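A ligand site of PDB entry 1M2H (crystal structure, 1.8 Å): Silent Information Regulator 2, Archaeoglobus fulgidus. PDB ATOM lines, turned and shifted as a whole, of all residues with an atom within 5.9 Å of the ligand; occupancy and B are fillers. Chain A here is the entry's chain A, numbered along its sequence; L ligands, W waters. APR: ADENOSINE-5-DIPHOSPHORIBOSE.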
ATOM      1  N   THR A  19      -5.443  16.852  13.649  1.00  0.00           N
ATOM      2  CA  THR A  19      -4.170  17.568  13.727  1.00  0.00           C
ATOM      3  C   THR A  19      -3.288  16.986  14.822  1.00  0.00           C
ATOM      4  O   THR A  19      -3.767  16.369  15.775  1.00  0.00           O
ATOM      5  CB  THR A  19      -4.359  19.080  14.023  1.00  0.00           C
ATOM      6  OG1 THR A  19      -4.942  19.262  15.309  1.00  0.00           O
ATOM      7  CG2 THR A  19      -5.228  19.743  12.954  1.00  0.00           C
ATOM      8  N   GLY A  20      -1.985  17.199  14.648  1.00  0.00           N
ATOM      9  CA  GLY A  20      -0.998  16.737  15.604  1.00  0.00           C
ATOM     10  C   GLY A  20      -0.065  17.881  15.960  1.00  0.00           C
ATOM     11  O   GLY A  20      -0.283  19.016  15.533  1.00  0.00           O
ATOM     12  N   ALA A  21       0.982  17.580  16.723  1.00  0.00           N
ATOM     13  CA  ALA A  21       1.946  18.574  17.191  1.00  0.00           C
ATOM     14  C   ALA A  21       2.554  19.471  16.114  1.00  0.00           C
ATOM     15  O   ALA A  21       2.987  20.591  16.402  1.00  0.00           O
ATOM     16  CB  ALA A  21       3.054  17.882  17.972  1.00  0.00           C
ATOM     17  N   GLY A  22       2.601  18.997  14.878  1.00  0.00           N
ATOM     18  CA  GLY A  22       3.163  19.791  13.804  1.00  0.00           C
ATOM     19  C   GLY A  22       2.399  21.072  13.525  1.00  0.00           C
ATOM     20  O   GLY A  22       2.951  22.040  13.025  1.00  0.00           O
ATOM     21  N   VAL A  23       1.108  21.090  13.861  1.00  0.00           N
ATOM     22  CA  VAL A  23       0.312  22.273  13.626  1.00  0.00           C
ATOM     23  C   VAL A  23       0.599  23.376  14.640  1.00  0.00           C
ATOM     24  O   VAL A  23       0.145  24.505  14.487  1.00  0.00           O
ATOM     25  CB  VAL A  23      -1.191  21.917  13.604  1.00  0.00           C
ATOM     26  CG1 VAL A  23      -2.038  23.163  13.458  1.00  0.00           C
ATOM     27  CG2 VAL A  23      -1.473  20.984  12.425  1.00  0.00           C
ATOM     28  N   ALA A  25       3.916  23.805  15.709  1.00  0.00           N
ATOM     29  CA  ALA A  25       5.332  24.098  15.513  1.00  0.00           C
ATOM     30  C   ALA A  25       5.597  25.543  15.132  1.00  0.00           C
ATOM     31  O   ALA A  25       6.551  26.160  15.621  1.00  0.00           O
ATOM     32  CB  ALA A  25       5.903  23.176  14.450  1.00  0.00           C
ATOM     33  N   GLU A  26       4.756  26.094  14.252  1.00  0.00           N
ATOM     34  CA  GLU A  26       4.944  27.472  13.808  1.00  0.00           C
ATOM     35  C   GLU A  26       4.532  28.510  14.856  1.00  0.00           C
ATOM     36  O   GLU A  26       4.563  29.715  14.597  1.00  0.00           O
ATOM     37  CB  GLU A  26       4.222  27.687  12.482  1.00  0.00           C
ATOM     38  CG  GLU A  26       4.851  26.847  11.363  1.00  0.00           C
ATOM     39  CD  GLU A  26       4.004  26.753  10.116  1.00  0.00           C
ATOM     40  OE1 GLU A  26       4.009  27.710   9.310  1.00  0.00           O
ATOM     41  OE2 GLU A  26       3.329  25.718   9.947  1.00  0.00           O
ATOM     42  N   THR A  31       7.795  19.927  18.313  1.00  0.00           N
ATOM     43  CA  THR A  31       6.989  18.713  18.219  1.00  0.00           C
ATOM     44  C   THR A  31       7.576  17.642  19.135  1.00  0.00           C
ATOM     45  O   THR A  31       8.587  17.867  19.786  1.00  0.00           O
ATOM     46  CB  THR A  31       6.955  18.187  16.781  1.00  0.00           C
ATOM     47  OG1 THR A  31       8.283  17.901  16.342  1.00  0.00           O
ATOM     48  CG2 THR A  31       6.320  19.206  15.856  1.00  0.00           C
ATOM     49  N   PHE A  32       6.943  16.484  19.170  1.00  0.00           N
ATOM     50  CA  PHE A  32       7.410  15.393  20.015  1.00  0.00           C
ATOM     51  C   PHE A  32       8.514  14.582  19.359  1.00  0.00           C
ATOM     52  O   PHE A  32       9.503  14.222  19.993  1.00  0.00           O
ATOM     53  CB  PHE A  32       6.259  14.469  20.395  1.00  0.00           C
ATOM     54  CG  PHE A  32       5.246  15.119  21.278  1.00  0.00           C
ATOM     55  CD1 PHE A  32       5.520  15.348  22.625  1.00  0.00           C
ATOM     56  CD2 PHE A  32       4.024  15.541  20.762  1.00  0.00           C
ATOM     57  CE1 PHE A  32       4.610  16.007  23.438  1.00  0.00           C
ATOM     58  CE2 PHE A  32       3.100  16.202  21.565  1.00  0.00           C
ATOM     59  CZ  PHE A  32       3.396  16.437  22.913  1.00  0.00           C
ATOM     60  N   ARG A  33       8.341  14.312  18.069  1.00  0.00           N
ATOM     61  CA  ARG A  33       9.316  13.525  17.338  1.00  0.00           C
ATOM     62  C   ARG A  33       9.968  14.318  16.219  1.00  0.00           C
ATOM     63  O   ARG A  33       9.456  15.364  15.811  1.00  0.00           O
ATOM     64  CB  ARG A  33       8.612  12.265  16.802  1.00  0.00           C
ATOM     65  CG  ARG A  33       7.897  11.509  17.918  1.00  0.00           C
ATOM     66  CD  ARG A  33       7.090  10.306  17.442  1.00  0.00           C
ATOM     67  NE  ARG A  33       6.484   9.596  18.562  1.00  0.00           N
ATOM     68  CZ  ARG A  33       5.441  10.034  19.262  1.00  0.00           C
ATOM     69  NH1 ARG A  33       4.966   9.321  20.270  1.00  0.00           N
ATOM     70  NH2 ARG A  33       4.849  11.188  18.947  1.00  0.00           N
ATOM     71  N   GLY A  34      11.105  13.827  15.743  1.00  0.00           N
ATOM     72  CA  GLY A  34      11.806  14.524  14.687  1.00  0.00           C
ATOM     73  C   GLY A  34      13.079  15.188  15.178  1.00  0.00           C
ATOM     74  O   GLY A  34      13.598  14.828  16.232  1.00  0.00           O
ATOM     75  N   TRP A  39      10.564  14.361  22.745  1.00  0.00           N
ATOM     76  CA  TRP A  39      10.823  12.977  23.170  1.00  0.00           C
ATOM     77  C   TRP A  39      12.238  12.524  22.822  1.00  0.00           C
ATOM     78  O   TRP A  39      12.645  11.425  23.178  1.00  0.00           O
ATOM     79  CB  TRP A  39       9.806  12.023  22.539  1.00  0.00           C
ATOM     80  CG  TRP A  39       8.401  12.126  23.088  1.00  0.00           C
ATOM     81  CD1 TRP A  39       7.269  11.589  22.530  1.00  0.00           C
ATOM     82  CD2 TRP A  39       7.975  12.742  24.309  1.00  0.00           C
ATOM     83  NE1 TRP A  39       6.175  11.837  23.323  1.00  0.00           N
ATOM     84  CE2 TRP A  39       6.579  12.546  24.426  1.00  0.00           C
ATOM     85  CE3 TRP A  39       8.636  13.453  25.328  1.00  0.00           C
ATOM     86  CZ2 TRP A  39       5.835  13.023  25.505  1.00  0.00           C
ATOM     87  CZ3 TRP A  39       7.892  13.929  26.407  1.00  0.00           C
ATOM     88  CH2 TRP A  39       6.504  13.711  26.486  1.00  0.00           C
ATOM     89  N   GLN A  98      -4.803  15.909  18.591  1.00  0.00           N
ATOM     90  CA  GLN A  98      -4.062  15.103  19.553  1.00  0.00           C
ATOM     91  C   GLN A  98      -3.294  16.077  20.445  1.00  0.00           C
ATOM     92  O   GLN A  98      -2.681  15.682  21.438  1.00  0.00           O
ATOM     93  CB  GLN A  98      -3.069  14.192  18.831  1.00  0.00           C
ATOM     94  CG  GLN A  98      -3.730  13.153  17.922  1.00  0.00           C
ATOM     95  CD  GLN A  98      -2.746  12.508  16.981  1.00  0.00           C
ATOM     96  OE1 GLN A  98      -1.994  11.608  17.361  1.00  0.00           O
ATOM     97  NE2 GLN A  98      -2.721  12.972  15.739  1.00  0.00           N
ATOM     98  N   ASN A  99      -3.340  17.351  20.072  1.00  0.00           N
ATOM     99  CA  ASN A  99      -2.630  18.384  20.813  1.00  0.00           C
ATOM    100  C   ASN A  99      -3.278  18.724  22.136  1.00  0.00           C
ATOM    101  O   ASN A  99      -4.506  18.728  22.252  1.00  0.00           O
ATOM    102  CB  ASN A  99      -2.513  19.655  19.954  1.00  0.00           C
ATOM    103  CG  ASN A  99      -1.765  19.414  18.663  1.00  0.00           C
ATOM    104  OD1 ASN A  99      -1.111  18.383  18.490  1.00  0.00           O
ATOM    105  ND2 ASN A  99      -1.843  20.364  17.738  1.00  0.00           N
ATOM    106  N   HIS A 116      -6.325  13.573  23.389  1.00  0.00           N
ATOM    107  CA  HIS A 116      -5.355  13.325  24.452  1.00  0.00           C
ATOM    108  C   HIS A 116      -5.410  14.292  25.628  1.00  0.00           C
ATOM    109  O   HIS A 116      -4.435  14.449  26.368  1.00  0.00           O
ATOM    110  CB  HIS A 116      -3.941  13.323  23.852  1.00  0.00           C
ATOM    111  CG  HIS A 116      -3.754  12.323  22.756  1.00  0.00           C
ATOM    112  ND1 HIS A 116      -2.646  12.307  21.942  1.00  0.00           N
ATOM    113  CD2 HIS A 116      -4.535  11.296  22.335  1.00  0.00           C
ATOM    114  CE1 HIS A 116      -2.755  11.315  21.066  1.00  0.00           C
ATOM    115  NE2 HIS A 116      -3.892  10.688  21.287  1.00  0.00           N
ATOM    116  N   VAL A 157      -3.641  12.759  28.578  1.00  0.00           N
ATOM    117  CA  VAL A 157      -3.550  11.299  28.514  1.00  0.00           C
ATOM    118  C   VAL A 157      -2.106  10.854  28.316  1.00  0.00           C
ATOM    119  O   VAL A 157      -1.419  11.289  27.381  1.00  0.00           O
ATOM    120  CB  VAL A 157      -4.407  10.748  27.333  1.00  0.00           C
ATOM    121  CG1 VAL A 157      -4.305   9.213  27.281  1.00  0.00           C
ATOM    122  CG2 VAL A 157      -5.855  11.178  27.491  1.00  0.00           C
ATOM    123  N   PHE A 159       0.957   7.623  28.097  1.00  0.00           N
ATOM    124  CA  PHE A 159       1.104   6.315  27.461  1.00  0.00           C
ATOM    125  C   PHE A 159       0.589   5.212  28.369  1.00  0.00           C
ATOM    126  O   PHE A 159       0.846   5.208  29.571  1.00  0.00           O
ATOM    127  CB  PHE A 159       2.571   6.043  27.116  1.00  0.00           C
ATOM    128  CG  PHE A 159       3.087   6.853  25.969  1.00  0.00           C
ATOM    129  CD1 PHE A 159       3.627   8.119  26.175  1.00  0.00           C
ATOM    130  CD2 PHE A 159       3.004   6.368  24.661  1.00  0.00           C
ATOM    131  CE1 PHE A 159       4.073   8.895  25.105  1.00  0.00           C
ATOM    132  CE2 PHE A 159       3.446   7.124  23.581  1.00  0.00           C
ATOM    133  CZ  PHE A 159       3.983   8.394  23.811  1.00  0.00           C
ATOM    134  N   ALA A 184      -3.143  16.890   9.314  1.00  0.00           N
ATOM    135  CA  ALA A 184      -2.013  17.794   9.347  1.00  0.00           C
ATOM    136  C   ALA A 184      -1.149  17.749  10.598  1.00  0.00           C
ATOM    137  O   ALA A 184      -1.651  17.690  11.720  1.00  0.00           O
ATOM    138  CB  ALA A 184      -2.516  19.225   9.132  1.00  0.00           C
ATOM    139  N   GLY A 185       0.163  17.789  10.380  1.00  0.00           N
ATOM    140  CA  GLY A 185       1.113  17.812  11.473  1.00  0.00           C
ATOM    141  C   GLY A 185       1.174  16.625  12.410  1.00  0.00           C
ATOM    142  O   GLY A 185       1.453  16.794  13.592  1.00  0.00           O
ATOM    143  N   THR A 186       0.940  15.426  11.912  1.00  0.00           N
ATOM    144  CA  THR A 186       0.999  14.265  12.779  1.00  0.00           C
ATOM    145  C   THR A 186       1.826  13.172  12.121  1.00  0.00           C
ATOM    146  O   THR A 186       1.759  12.978  10.917  1.00  0.00           O
ATOM    147  CB  THR A 186      -0.409  13.741  13.155  1.00  0.00           C
ATOM    148  OG1 THR A 186      -0.282  12.591  14.001  1.00  0.00           O
ATOM    149  CG2 THR A 186      -1.205  13.375  11.907  1.00  0.00           C
ATOM    150  N   SER A 187       2.631  12.490  12.943  1.00  0.00           N
ATOM    151  CA  SER A 187       3.509  11.429  12.463  1.00  0.00           C
ATOM    152  C   SER A 187       2.829  10.104  12.133  1.00  0.00           C
ATOM    153  O   SER A 187       3.478   9.189  11.643  1.00  0.00           O
ATOM    154  CB  SER A 187       4.636  11.207  13.488  1.00  0.00           C
ATOM    155  OG  SER A 187       4.104  10.909  14.770  1.00  0.00           O
ATOM    156  N   ALA A 188       1.528  10.015  12.421  1.00  0.00           N
ATOM    157  CA  ALA A 188       0.750   8.817  12.126  1.00  0.00           C
ATOM    158  C   ALA A 188       1.287   7.503  12.707  1.00  0.00           C
ATOM    159  O   ALA A 188       1.303   6.475  12.018  1.00  0.00           O
ATOM    160  CB  ALA A 188       0.573   8.668  10.618  1.00  0.00           C
ATOM    161  N   VAL A 189       1.731   7.529  13.959  1.00  0.00           N
ATOM    162  CA  VAL A 189       2.239   6.331  14.596  1.00  0.00           C
ATOM    163  C   VAL A 189       1.512   5.999  15.898  1.00  0.00           C
ATOM    164  O   VAL A 189       1.250   4.834  16.189  1.00  0.00           O
ATOM    165  CB  VAL A 189       3.761   6.439  14.897  1.00  0.00           C
ATOM    166  CG1 VAL A 189       4.535   6.435  13.591  1.00  0.00           C
ATOM    167  CG2 VAL A 189       4.064   7.699  15.687  1.00  0.00           C
ATOM    168  N   VAL A 190       1.170   7.027  16.657  1.00  0.00           N
ATOM    169  CA  VAL A 190       0.482   6.840  17.929  1.00  0.00           C
ATOM    170  C   VAL A 190      -0.981   6.425  17.753  1.00  0.00           C
ATOM    171  O   VAL A 190      -1.739   7.092  17.041  1.00  0.00           O
ATOM    172  CB  VAL A 190       0.534   8.114  18.788  1.00  0.00           C
ATOM    173  CG1 VAL A 190      -0.218   7.913  20.093  1.00  0.00           C
ATOM    174  CG2 VAL A 190       1.989   8.468  19.076  1.00  0.00           C
ATOM    175  N   ILE A 210      -1.052  16.805   5.251  1.00  0.00           N
ATOM    176  CA  ILE A 210      -0.211  18.002   5.201  1.00  0.00           C
ATOM    177  C   ILE A 210       0.898  17.764   6.206  1.00  0.00           C
ATOM    178  O   ILE A 210       0.672  17.742   7.418  1.00  0.00           O
ATOM    179  CB  ILE A 210      -0.986  19.266   5.611  1.00  0.00           C
ATOM    180  CG1 ILE A 210      -2.204  19.450   4.699  1.00  0.00           C
ATOM    181  CG2 ILE A 210      -0.070  20.483   5.532  1.00  0.00           C
ATOM    182  CD1 ILE A 210      -1.856  19.528   3.245  1.00  0.00           C
ATOM    183  N   ASN A 211       2.129  17.605   5.710  1.00  0.00           N
ATOM    184  CA  ASN A 211       3.263  17.315   6.576  1.00  0.00           C
ATOM    185  C   ASN A 211       4.552  17.459   5.772  1.00  0.00           C
ATOM    186  O   ASN A 211       4.631  17.003   4.628  1.00  0.00           O
ATOM    187  CB  ASN A 211       3.119  15.868   7.068  1.00  0.00           C
ATOM    188  CG  ASN A 211       3.988  15.564   8.275  1.00  0.00           C
ATOM    189  OD1 ASN A 211       5.179  15.859   8.290  1.00  0.00           O
ATOM    190  ND2 ASN A 211       3.381  14.950   9.285  1.00  0.00           N
ATOM    191  N   PRO A 212       5.589  18.090   6.349  1.00  0.00           N
ATOM    192  CA  PRO A 212       6.851  18.245   5.625  1.00  0.00           C
ATOM    193  C   PRO A 212       7.550  16.900   5.406  1.00  0.00           C
ATOM    194  O   PRO A 212       8.434  16.789   4.565  1.00  0.00           O
ATOM    195  CB  PRO A 212       7.659  19.187   6.512  1.00  0.00           C
ATOM    196  CG  PRO A 212       7.097  18.934   7.888  1.00  0.00           C
ATOM    197  CD  PRO A 212       5.618  18.831   7.620  1.00  0.00           C
ATOM    198  N   ASP A 213       7.150  15.895   6.174  1.00  0.00           N
ATOM    199  CA  ASP A 213       7.716  14.561   6.061  1.00  0.00           C
ATOM    200  C   ASP A 213       6.663  13.578   5.580  1.00  0.00           C
ATOM    201  O   ASP A 213       5.467  13.844   5.661  1.00  0.00           O
ATOM    202  CB  ASP A 213       8.229  14.040   7.404  1.00  0.00           C
ATOM    203  CG  ASP A 213       9.392  14.834   7.956  1.00  0.00           C
ATOM    204  OD1 ASP A 213      10.124  15.465   7.158  1.00  0.00           O
ATOM    205  OD2 ASP A 213       9.584  14.825   9.185  1.00  0.00           O
ATOM    206  N   THR A 215       4.834   9.942   6.009  1.00  0.00           N
ATOM    207  CA  THR A 215       4.487   9.146   7.187  1.00  0.00           C
ATOM    208  C   THR A 215       3.905   7.796   6.774  1.00  0.00           C
ATOM    209  O   THR A 215       3.788   7.496   5.588  1.00  0.00           O
ATOM    210  CB  THR A 215       3.431   9.867   8.060  1.00  0.00           C
ATOM    211  OG1 THR A 215       2.138   9.745   7.438  1.00  0.00           O
ATOM    212  CG2 THR A 215       3.767  11.339   8.229  1.00  0.00           C
ATOM    213  N   GLY A 227       4.821  20.276   3.054  1.00  0.00           N
ATOM    214  CA  GLY A 227       5.021  21.665   3.425  1.00  0.00           C
ATOM    215  C   GLY A 227       4.525  21.919   4.833  1.00  0.00           C
ATOM    216  O   GLY A 227       3.899  21.048   5.444  1.00  0.00           O
ATOM    217  N   LYS A 228       4.808  23.116   5.352  1.00  0.00           N
ATOM    218  CA  LYS A 228       4.379  23.483   6.692  1.00  0.00           C
ATOM    219  C   LYS A 228       2.891  23.784   6.687  1.00  0.00           C
ATOM    220  O   LYS A 228       2.369  24.377   5.747  1.00  0.00           O
ATOM    221  CB  LYS A 228       5.159  24.700   7.180  1.00  0.00           C
ATOM    222  CG  LYS A 228       6.651  24.449   7.315  1.00  0.00           C
ATOM    223  CD  LYS A 228       7.399  25.679   7.832  1.00  0.00           C
ATOM    224  CE  LYS A 228       8.867  25.343   8.064  1.00  0.00           C
ATOM    225  NZ  LYS A 228       9.661  26.531   8.504  1.00  0.00           N
ATOM    226  N   ALA A 229       2.203  23.380   7.742  1.00  0.00           N
ATOM    227  CA  ALA A 229       0.758  23.581   7.846  1.00  0.00           C
ATOM    228  C   ALA A 229       0.328  25.034   7.718  1.00  0.00           C
ATOM    229  O   ALA A 229      -0.702  25.334   7.130  1.00  0.00           O
ATOM    230  CB  ALA A 229       0.257  23.008   9.163  1.00  0.00           C
ATOM    231  N   GLY A 230       1.111  25.943   8.289  1.00  0.00           N
ATOM    232  CA  GLY A 230       0.778  27.353   8.234  1.00  0.00           C
ATOM    233  C   GLY A 230       0.658  27.862   6.806  1.00  0.00           C
ATOM    234  O   GLY A 230      -0.358  28.456   6.438  1.00  0.00           O
HETATM  235  N1  APR L   1       3.496  21.834   9.688  1.00  0.00           N
HETATM  236  C2  APR L   1       2.923  20.559   9.605  1.00  0.00           C
HETATM  237  N3  APR L   1       3.580  19.459  10.167  1.00  0.00           N
HETATM  238  C4  APR L   1       4.809  19.657  10.808  1.00  0.00           C
HETATM  239  C5  APR L   1       5.383  20.923  10.897  1.00  0.00           C
HETATM  240  C6  APR L   1       4.725  22.054  10.327  1.00  0.00           C
HETATM  241  N6  APR L   1       5.251  23.291  10.402  1.00  0.00           N
HETATM  242  N7  APR L   1       6.528  20.810  11.551  1.00  0.00           N
HETATM  243  C8  APR L   1       6.669  19.492  11.869  1.00  0.00           C
HETATM  244  N9  APR L   1       5.583  18.673  11.422  1.00  0.00           N
HETATM  245  C1' APR L   1       5.239  17.291  11.501  1.00  0.00           C
HETATM  246  C2' APR L   1       6.374  16.419  11.602  1.00  0.00           C
HETATM  247  O2' APR L   1       7.040  16.189  10.476  1.00  0.00           O
HETATM  248  C3' APR L   1       5.813  15.284  12.253  1.00  0.00           C
HETATM  249  O3' APR L   1       5.456  14.307  11.393  1.00  0.00           O
HETATM  250  O4' APR L   1       4.579  17.072  12.643  1.00  0.00           O
HETATM  251  C4' APR L   1       4.645  15.753  12.925  1.00  0.00           C
HETATM  252  C5' APR L   1       4.635  15.619  14.385  1.00  0.00           C
HETATM  253  O5' APR L   1       4.718  14.338  14.775  1.00  0.00           O
HETATM  254  PA  APR L   1       4.693  14.100  16.394  1.00  0.00           P
HETATM  255  O1A APR L   1       5.850  14.918  17.112  1.00  0.00           O
HETATM  256  O2A APR L   1       4.837  12.548  16.688  1.00  0.00           O
HETATM  257  O3A APR L   1       3.310  14.700  16.972  1.00  0.00           O
HETATM  258  PB  APR L   1       1.941  13.811  17.044  1.00  0.00           P
HETATM  259  O1B APR L   1       1.676  12.961  15.747  1.00  0.00           O
HETATM  260  O2B APR L   1       0.767  14.822  17.309  1.00  0.00           O
HETATM  261  O5D APR L   1       2.135  12.876  18.342  1.00  0.00           O
HETATM  262  C5D APR L   1       1.138  12.061  18.662  1.00  0.00           C
HETATM  263  O4D APR L   1       2.251  11.449  20.637  1.00  0.00           O
HETATM  264  O1D APR L   1       3.395  11.405  22.562  1.00  0.00           O
HETATM  265  C1D APR L   1       2.769  12.202  21.537  1.00  0.00           C
HETATM  266  O2D APR L   1       0.637  12.407  23.019  1.00  0.00           O
HETATM  267  C2D APR L   1       1.552  12.828  22.165  1.00  0.00           C
HETATM  268  O3D APR L   1      -0.193  13.754  20.905  1.00  0.00           O
HETATM  269  C3D APR L   1       0.995  13.157  20.875  1.00  0.00           C
HETATM  270  C4D APR L   1       1.123  11.946  20.136  1.00  0.00           C
HETATM  271  O   HOH W   1      -0.090  16.434  22.785  1.00  0.00           O
HETATM  272  O   HOH W   2       0.026  16.083  19.545  1.00  0.00           O
HETATM  273  O   HOH W   3       8.943  22.055  12.280  1.00  0.00           O
HETATM  274  O   HOH W   4       1.625   9.894  15.734  1.00  0.00           O
HETATM  275  O   HOH W   5       8.873  15.024  13.378  1.00  0.00           O
HETATM  276  O   HOH W   6       7.769  24.291  11.375  1.00  0.00           O
HETATM  277  O   HOH W   7       9.121  17.833  13.572  1.00  0.00           O
HETATM  278  O   HOH W   8       7.625  12.953  10.584  1.00  0.00           O
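Water W2 lies within hydrogen-bond range of O2B of the ligand (2.7 Å), OD1 of Asn 99 (2.8 Å), O of Gln 98 (3.3 Å) and N of Ala 21 (3.3 Å).
Water W8 bridges an oxygen (O3') of the ligand and the side-chain carboxylate of Asp 213.
Water W1 lies within hydrogen-bond range of O of Gln 98 (3.0 Å) and O3D of the ligand (3.3 Å).
Water W7 lies within hydrogen-bond range of OG1 of Thr 31 (2.9 Å) and O of Arg 33 (3.3 Å).
O of Gly 22 lies close to N1 of the ligand, 3.4 Å away.
The backbone carbonyl oxygen (O) of Gly 185 lies close to an oxygen (O4') of the ligand, 3.3 Å away.
Residues that only touch the ligand: Gly 20, Phe 159, Pro 212, Val 190, Thr 31, Lys 228 and Ala 25.
Hydrophobic or aromatic side chains within 4 Å of the ligand: Ala 21, Ala 25, Phe 32, Trp 39, His 116, Phe 159, Val 190, Pro 212 and Ala 229.
Within 4 Å of the ligand: Gly 20, Ala 21, Gly 22, Ala 25, Glu 26, Thr 31, Phe 32, Arg 33, Trp 39, Gln 98, His 116, Phe 159, Gly 185, Thr 186, Ser 187, Val 190, Asn 211, Pro 212, Asp 213, Lys 228 and Ala 229.
The nearest printed residue that does not touch the ligand is Asn 99 (4.2 Å).
OG1 of Thr 186 sits at hydrogen-bond distance from NE2 of Gln 98, at 3.0 Å.
The backbone NH of Ala 229 lies within hydrogen-bond range of the side-chain carboxylate of Glu 26 (3.4 Å).
ND2 of Asn 99 lies within hydrogen-bond range of O of Gly 20 (3.0 Å).
O of Thr 186 is in hydrogen-bond range of ND2 of Asn 211 (3.0 Å).
The side-chain amide oxygen of Asn 211 is in hydrogen-bond range of the backbone NH of Asp 213 (2.9 Å).
The side-chain carboxylate (OE2) of Glu 26 is in hydrogen-bond range of the backbone NH (N) of Gly 230 (2.8 Å).
ND1 of His 116 is in hydrogen-bond range of O of Gln 98 (3.4 Å).
The backbone carbonyl oxygen of Ile 210 lies within hydrogen-bond range of the backbone NH of Gly 185 (3.0 Å).
O3D of the ligand is in hydrogen-bond range of ND1 of His 116, 3.0 Å away.
An oxygen (O2A) of the ligand is in salt-bridge range of the guanidinium group of Arg 33 (2.6 Å).
OD2 of Asp 213 sits at hydrogen-bond distance from O2' of the ligand, 3.2 Å away.
N of Ala 21 sits at hydrogen-bond distance from O2B of the ligand.
N of Ala 229 sits at hydrogen-bond distance from N1 of the ligand (2.8 Å).
The indole nitrogen (NE1) of Trp 39 sits at hydrogen-bond distance from an oxygen (O1D) of the ligand.
The side-chain carboxylate (OE2) of Glu 26 is in hydrogen-bond range of a nitrogen (N6) of the ligand, at 3.1 Å.
O1A of the ligand lies within hydrogen-bond range of N of Arg 33.
O2A of the ligand lies within hydrogen-bond range of OG of Ser 187.
N of Ser 187 lies within hydrogen-bond range of O1B of the ligand, at 3.0 Å.
An oxygen (O2') of the ligand lies within hydrogen-bond range of the side-chain amide oxygen (OD1) of Asn 211 (2.9 Å).
The backbone carbonyl oxygen (O) of Gln 98 sits at hydrogen-bond distance from an oxygen (O3D) of the ligand.
OG1 of Thr 186 is in hydrogen-bond range of O1B of the ligand (2.6 Å).
O1A of the ligand lies within hydrogen-bond range of N of Phe 32 (2.8 Å).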
